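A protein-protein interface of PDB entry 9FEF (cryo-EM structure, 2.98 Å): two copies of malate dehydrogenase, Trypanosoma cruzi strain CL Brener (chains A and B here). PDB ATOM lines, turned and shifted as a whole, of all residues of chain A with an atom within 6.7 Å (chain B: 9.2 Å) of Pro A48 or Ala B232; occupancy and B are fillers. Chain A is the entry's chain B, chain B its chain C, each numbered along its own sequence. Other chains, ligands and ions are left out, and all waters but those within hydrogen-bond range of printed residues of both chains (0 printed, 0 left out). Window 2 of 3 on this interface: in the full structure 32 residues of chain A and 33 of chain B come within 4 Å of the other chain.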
ATOM      1  N   ASP A  43      19.942 -16.740 -15.821  1.00  0.00           N
ATOM      2  CA  ASP A  43      19.990 -17.800 -14.825  1.00  0.00           C
ATOM      3  C   ASP A  43      19.927 -19.141 -15.538  1.00  0.00           C
ATOM      4  O   ASP A  43      19.508 -19.231 -16.694  1.00  0.00           O
ATOM      5  CB  ASP A  43      18.857 -17.686 -13.803  1.00  0.00           C
ATOM      6  CG  ASP A  43      19.204 -18.350 -12.483  1.00  0.00           C
ATOM      7  OD1 ASP A  43      20.404 -18.417 -12.149  1.00  0.00           O
ATOM      8  OD2 ASP A  43      18.282 -18.818 -11.787  1.00  0.00           O
ATOM      9  N   VAL A  45      18.033 -21.722 -14.713  1.00  0.00           N
ATOM     10  CA  VAL A  45      16.623 -22.072 -14.848  1.00  0.00           C
ATOM     11  C   VAL A  45      15.779 -20.906 -14.351  1.00  0.00           C
ATOM     12  O   VAL A  45      16.109 -20.269 -13.346  1.00  0.00           O
ATOM     13  CB  VAL A  45      16.262 -23.371 -14.090  1.00  0.00           C
ATOM     14  CG1 VAL A  45      17.077 -24.548 -14.600  1.00  0.00           C
ATOM     15  CG2 VAL A  45      16.478 -23.205 -12.597  1.00  0.00           C
ATOM     16  N   GLY A  46      14.700 -20.614 -15.071  1.00  0.00           N
ATOM     17  CA  GLY A  46      13.726 -19.641 -14.623  1.00  0.00           C
ATOM     18  C   GLY A  46      13.938 -18.220 -15.087  1.00  0.00           C
ATOM     19  O   GLY A  46      13.295 -17.313 -14.545  1.00  0.00           O
ATOM     20  N   ALA A  47      14.813 -17.986 -16.059  1.00  0.00           N
ATOM     21  CA  ALA A  47      15.046 -16.628 -16.539  1.00  0.00           C
ATOM     22  C   ALA A  47      13.946 -16.156 -17.492  1.00  0.00           C
ATOM     23  O   ALA A  47      13.530 -14.992 -17.396  1.00  0.00           O
ATOM     24  CB  ALA A  47      16.423 -16.516 -17.202  1.00  0.00           C
ATOM     25  N   PRO A  48      13.462 -16.982 -18.431  1.00  0.00           N
ATOM     26  CA  PRO A  48      12.331 -16.536 -19.264  1.00  0.00           C
ATOM     27  C   PRO A  48      11.109 -16.117 -18.470  1.00  0.00           C
ATOM     28  O   PRO A  48      10.455 -15.136 -18.845  1.00  0.00           O
ATOM     29  CB  PRO A  48      12.020 -17.759 -20.137  1.00  0.00           C
ATOM     30  CG  PRO A  48      13.226 -18.587 -20.127  1.00  0.00           C
ATOM     31  CD  PRO A  48      14.129 -18.161 -19.016  1.00  0.00           C
ATOM     32  N   GLY A  49      10.782 -16.816 -17.388  1.00  0.00           N
ATOM     33  CA  GLY A  49       9.614 -16.512 -16.593  1.00  0.00           C
ATOM     34  C   GLY A  49       9.688 -15.225 -15.813  1.00  0.00           C
ATOM     35  O   GLY A  49       8.643 -14.677 -15.449  1.00  0.00           O
ATOM     36  N   VAL A  50      10.887 -14.722 -15.541  1.00  0.00           N
ATOM     37  CA  VAL A  50      11.072 -13.425 -14.909  1.00  0.00           C
ATOM     38  C   VAL A  50      11.186 -12.317 -15.947  1.00  0.00           C
ATOM     39  O   VAL A  50      10.659 -11.218 -15.755  1.00  0.00           O
ATOM     40  CB  VAL A  50      12.312 -13.465 -13.988  1.00  0.00           C
ATOM     41  CG1 VAL A  50      12.912 -12.081 -13.805  1.00  0.00           C
ATOM     42  CG2 VAL A  50      11.959 -14.081 -12.645  1.00  0.00           C
ATOM     43  N   ALA A  51      11.859 -12.610 -17.063  1.00  0.00           N
ATOM     44  CA  ALA A  51      11.954 -11.640 -18.148  1.00  0.00           C
ATOM     45  C   ALA A  51      10.582 -11.305 -18.711  1.00  0.00           C
ATOM     46  O   ALA A  51      10.271 -10.131 -18.939  1.00  0.00           O
ATOM     47  CB  ALA A  51      12.867 -12.172 -19.248  1.00  0.00           C
ATOM     48  N   ALA A  52       9.745 -12.313 -18.947  1.00  0.00           N
ATOM     49  CA  ALA A  52       8.364 -12.040 -19.337  1.00  0.00           C
ATOM     50  C   ALA A  52       7.457 -11.985 -18.115  1.00  0.00           C
ATOM     51  O   ALA A  52       6.367 -12.548 -18.080  1.00  0.00           O
ATOM     52  CB  ALA A  52       7.885 -13.091 -20.329  1.00  0.00           C
ATOM     53  N   ASP A  53       7.931 -11.298 -17.102  1.00  0.00           N
ATOM     54  CA  ASP A  53       7.205 -10.833 -15.929  1.00  0.00           C
ATOM     55  C   ASP A  53       7.502  -9.375 -15.635  1.00  0.00           C
ATOM     56  O   ASP A  53       6.601  -8.635 -15.237  1.00  0.00           O
ATOM     57  CB  ASP A  53       7.560 -11.695 -14.707  1.00  0.00           C
ATOM     58  CG  ASP A  53       6.499 -11.650 -13.632  1.00  0.00           C
ATOM     59  OD1 ASP A  53       5.653 -10.736 -13.663  1.00  0.00           O
ATOM     60  OD2 ASP A  53       6.514 -12.530 -12.748  1.00  0.00           O
ATOM     61  N   HIS A  66      17.133 -10.779 -21.902  1.00  0.00           N
ATOM     62  CA  HIS A  66      17.356 -12.002 -21.145  1.00  0.00           C
ATOM     63  C   HIS A  66      18.036 -13.038 -22.025  1.00  0.00           C
ATOM     64  O   HIS A  66      17.988 -12.971 -23.255  1.00  0.00           O
ATOM     65  CB  HIS A  66      16.047 -12.558 -20.575  1.00  0.00           C
ATOM     66  CG  HIS A  66      15.339 -13.514 -21.486  1.00  0.00           C
ATOM     67  ND1 HIS A  66      14.390 -13.109 -22.399  1.00  0.00           N
ATOM     68  CD2 HIS A  66      15.427 -14.860 -21.609  1.00  0.00           C
ATOM     69  CE1 HIS A  66      13.933 -14.161 -23.053  1.00  0.00           C
ATOM     70  NE2 HIS A  66      14.548 -15.236 -22.594  1.00  0.00           N
ATOM     71  N   ALA A  67      18.678 -13.998 -21.365  1.00  0.00           N
ATOM     72  CA  ALA A  67      19.299 -15.134 -22.028  1.00  0.00           C
ATOM     73  C   ALA A  67      18.882 -16.395 -21.295  1.00  0.00           C
ATOM     74  O   ALA A  67      18.969 -16.458 -20.066  1.00  0.00           O
ATOM     75  CB  ALA A  67      20.825 -15.011 -22.052  1.00  0.00           C
ATOM     76  N   ALA A  68      18.425 -17.392 -22.047  1.00  0.00           N
ATOM     77  CA  ALA A  68      17.951 -18.621 -21.437  1.00  0.00           C
ATOM     78  C   ALA A  68      19.116 -19.416 -20.858  1.00  0.00           C
ATOM     79  O   ALA A  68      20.275 -19.246 -21.241  1.00  0.00           O
ATOM     80  CB  ALA A  68      17.190 -19.468 -22.455  1.00  0.00           C
ATOM     81  N   GLY A  69      18.789 -20.300 -19.923  1.00  0.00           N
ATOM     82  CA  GLY A  69      19.789 -21.152 -19.316  1.00  0.00           C
ATOM     83  C   GLY A  69      20.194 -22.287 -20.229  1.00  0.00           C
ATOM     84  O   GLY A  69      20.311 -22.103 -21.444  1.00  0.00           O
ATOM     85  N   ALA B 225      -2.799 -11.667 -21.699  1.00  0.00           N
ATOM     86  CA  ALA B 225      -1.401 -11.543 -21.304  1.00  0.00           C
ATOM     87  C   ALA B 225      -1.068 -12.335 -20.048  1.00  0.00           C
ATOM     88  O   ALA B 225       0.110 -12.612 -19.803  1.00  0.00           O
ATOM     89  CB  ALA B 225      -1.037 -10.074 -21.085  1.00  0.00           C
ATOM     90  N   GLY B 226      -2.071 -12.695 -19.244  1.00  0.00           N
ATOM     91  CA  GLY B 226      -1.797 -13.443 -18.029  1.00  0.00           C
ATOM     92  C   GLY B 226      -1.275 -14.842 -18.295  1.00  0.00           C
ATOM     93  O   GLY B 226      -0.319 -15.287 -17.655  1.00  0.00           O
ATOM     94  N   THR B 227      -1.893 -15.554 -19.240  1.00  0.00           N
ATOM     95  CA  THR B 227      -1.476 -16.918 -19.542  1.00  0.00           C
ATOM     96  C   THR B 227      -0.151 -16.969 -20.290  1.00  0.00           C
ATOM     97  O   THR B 227       0.497 -18.020 -20.305  1.00  0.00           O
ATOM     98  CB  THR B 227      -2.551 -17.634 -20.359  1.00  0.00           C
ATOM     99  OG1 THR B 227      -2.326 -17.399 -21.754  1.00  0.00           O
ATOM    100  CG2 THR B 227      -3.933 -17.129 -19.982  1.00  0.00           C
ATOM    101  N   GLU B 228       0.260 -15.863 -20.910  1.00  0.00           N
ATOM    102  CA  GLU B 228       1.554 -15.827 -21.585  1.00  0.00           C
ATOM    103  C   GLU B 228       2.696 -16.011 -20.593  1.00  0.00           C
ATOM    104  O   GLU B 228       3.685 -16.690 -20.892  1.00  0.00           O
ATOM    105  CB  GLU B 228       1.696 -14.513 -22.351  1.00  0.00           C
ATOM    106  CG  GLU B 228       3.117 -14.117 -22.685  1.00  0.00           C
ATOM    107  CD  GLU B 228       3.241 -12.638 -22.985  1.00  0.00           C
ATOM    108  OE1 GLU B 228       2.567 -12.162 -23.923  1.00  0.00           O
ATOM    109  OE2 GLU B 228       4.010 -11.950 -22.283  1.00  0.00           O
ATOM    110  N   VAL B 229       2.572 -15.416 -19.405  1.00  0.00           N
ATOM    111  CA  VAL B 229       3.594 -15.582 -18.373  1.00  0.00           C
ATOM    112  C   VAL B 229       3.686 -17.042 -17.948  1.00  0.00           C
ATOM    113  O   VAL B 229       4.780 -17.599 -17.805  1.00  0.00           O
ATOM    114  CB  VAL B 229       3.298 -14.666 -17.172  1.00  0.00           C
ATOM    115  CG1 VAL B 229       4.310 -14.897 -16.064  1.00  0.00           C
ATOM    116  CG2 VAL B 229       3.280 -13.211 -17.600  1.00  0.00           C
ATOM    117  N   VAL B 230       2.533 -17.682 -17.738  1.00  0.00           N
ATOM    118  CA  VAL B 230       2.518 -19.086 -17.331  1.00  0.00           C
ATOM    119  C   VAL B 230       3.117 -19.964 -18.422  1.00  0.00           C
ATOM    120  O   VAL B 230       3.840 -20.925 -18.137  1.00  0.00           O
ATOM    121  CB  VAL B 230       1.086 -19.523 -16.974  1.00  0.00           C
ATOM    122  CG1 VAL B 230       1.086 -20.930 -16.408  1.00  0.00           C
ATOM    123  CG2 VAL B 230       0.470 -18.551 -15.985  1.00  0.00           C
ATOM    124  N   LYS B 231       2.819 -19.655 -19.685  1.00  0.00           N
ATOM    125  CA  LYS B 231       3.414 -20.403 -20.787  1.00  0.00           C
ATOM    126  C   LYS B 231       4.928 -20.234 -20.812  1.00  0.00           C
ATOM    127  O   LYS B 231       5.664 -21.196 -21.057  1.00  0.00           O
ATOM    128  CB  LYS B 231       2.797 -19.960 -22.114  1.00  0.00           C
ATOM    129  CG  LYS B 231       3.579 -20.386 -23.344  1.00  0.00           C
ATOM    130  CD  LYS B 231       2.722 -20.311 -24.600  1.00  0.00           C
ATOM    131  CE  LYS B 231       2.041 -18.959 -24.730  1.00  0.00           C
ATOM    132  NZ  LYS B 231       2.841 -18.006 -25.549  1.00  0.00           N
ATOM    133  N   ALA B 232       5.413 -19.017 -20.557  1.00  0.00           N
ATOM    134  CA  ALA B 232       6.849 -18.775 -20.486  1.00  0.00           C
ATOM    135  C   ALA B 232       7.486 -19.344 -19.226  1.00  0.00           C
ATOM    136  O   ALA B 232       8.713 -19.469 -19.175  1.00  0.00           O
ATOM    137  CB  ALA B 232       7.137 -17.274 -20.566  1.00  0.00           C
ATOM    138  N   LYS B 233       6.690 -19.691 -18.220  1.00  0.00           N
ATOM    139  CA  LYS B 233       7.187 -20.257 -16.974  1.00  0.00           C
ATOM    140  C   LYS B 233       7.071 -21.774 -16.937  1.00  0.00           C
ATOM    141  O   LYS B 233       7.288 -22.377 -15.881  1.00  0.00           O
ATOM    142  CB  LYS B 233       6.437 -19.644 -15.790  1.00  0.00           C
ATOM    143  CG  LYS B 233       7.309 -19.323 -14.594  1.00  0.00           C
ATOM    144  CD  LYS B 233       6.508 -18.627 -13.510  1.00  0.00           C
ATOM    145  CE  LYS B 233       6.555 -17.119 -13.677  1.00  0.00           C
ATOM    146  NZ  LYS B 233       7.555 -16.484 -12.776  1.00  0.00           N
ATOM    147  N   ALA B 234       6.726 -22.401 -18.066  1.00  0.00           N
ATOM    148  CA  ALA B 234       6.554 -23.851 -18.167  1.00  0.00           C
ATOM    149  C   ALA B 234       5.485 -24.367 -17.209  1.00  0.00           C
ATOM    150  O   ALA B 234       5.562 -25.499 -16.726  1.00  0.00           O
ATOM    151  CB  ALA B 234       7.877 -24.589 -17.944  1.00  0.00           C
ATOM    152  N   GLY B 235       4.477 -23.544 -16.930  1.00  0.00           N
ATOM    153  CA  GLY B 235       3.390 -23.955 -16.058  1.00  0.00           C
ATOM    154  C   GLY B 235       3.784 -24.133 -14.610  1.00  0.00           C
ATOM    155  O   GLY B 235       3.054 -24.780 -13.852  1.00  0.00           O
ATOM    156  N   ARG B 236       4.919 -23.570 -14.200  1.00  0.00           N
ATOM    157  CA  ARG B 236       5.407 -23.717 -12.836  1.00  0.00           C
ATOM    158  C   ARG B 236       4.929 -22.613 -11.902  1.00  0.00           C
ATOM    159  O   ARG B 236       5.184 -22.694 -10.696  1.00  0.00           O
ATOM    160  CB  ARG B 236       6.941 -23.759 -12.823  1.00  0.00           C
ATOM    161  CG  ARG B 236       7.528 -25.158 -12.904  1.00  0.00           C
ATOM    162  CD  ARG B 236       8.976 -25.121 -13.368  1.00  0.00           C
ATOM    163  NE  ARG B 236       9.559 -23.791 -13.228  1.00  0.00           N
ATOM    164  CZ  ARG B 236      10.733 -23.429 -13.730  1.00  0.00           C
ATOM    165  NH1 ARG B 236      11.487 -24.278 -14.408  1.00  0.00           N
ATOM    166  NH2 ARG B 236      11.160 -22.183 -13.546  1.00  0.00           N
ATOM    167  N   GLY B 237       4.253 -21.591 -12.420  1.00  0.00           N
ATOM    168  CA  GLY B 237       3.770 -20.511 -11.584  1.00  0.00           C
ATOM    169  C   GLY B 237       2.882 -19.532 -12.323  1.00  0.00           C
ATOM    170  O   GLY B 237       2.077 -19.930 -13.168  1.00  0.00           O
ATOM    171  N   SER B 238       3.023 -18.248 -12.012  1.00  0.00           N
ATOM    172  CA  SER B 238       2.234 -17.197 -12.643  1.00  0.00           C
ATOM    173  C   SER B 238       2.979 -15.878 -12.471  1.00  0.00           C
ATOM    174  O   SER B 238       4.104 -15.844 -11.960  1.00  0.00           O
ATOM    175  CB  SER B 238       0.823 -17.143 -12.050  1.00  0.00           C
ATOM    176  OG  SER B 238       0.755 -16.206 -10.991  1.00  0.00           O
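The side-chain amino group (NZ) of Lys B233 lies within hydrogen-bond range of the backbone carbonyl oxygen (O) of Gly A49 (3.4 Å).
Arg B236 touches Gly A46.
Pro A48 touches Ala B232.
Gly A49 touches Ala B232.
CG2 of Val B229 touches O of Ala A52 (3.2 Å).
Gly A46 touches just one residue of chain B: Arg B236.
Gly A49 touches two residues of chain B.
Ala A51 touches none of the printed residues of chain B.
Of chain B, only Val B229 (3.2 Å) comes within 4 Å of Ala A52.
Of chain A, only Pro A48 and Gly A49 come within 4 Å of Ala B232.
Of the printed residues of chain A, Lys B233 touches Gly A49.
Of the printed residues of chain A, Arg B236 touches Gly A46 (3.8 Å).
The nearest residue of chain B that does not touch Pro A48 is Lys B233 (5.7 Å).
The nearest printed residue of chain A that does not touch Arg B236 is Val A45 (4.9 Å).
Printed residues of chain A that touch a printed residue of chain B: Gly A46, Pro A48, Gly A49 and Ala A52.
Along chain A the printed residues that touch a printed residue of chain B span positions 46 to 52.
Among the printed residues, 5 pairs touch across the chains.
Among the printed residues, no Asp or Glu carboxylate lies within 4 Å of a Lys or Arg side-chain nitrogen of the other chain.
No position is printed for both chains.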
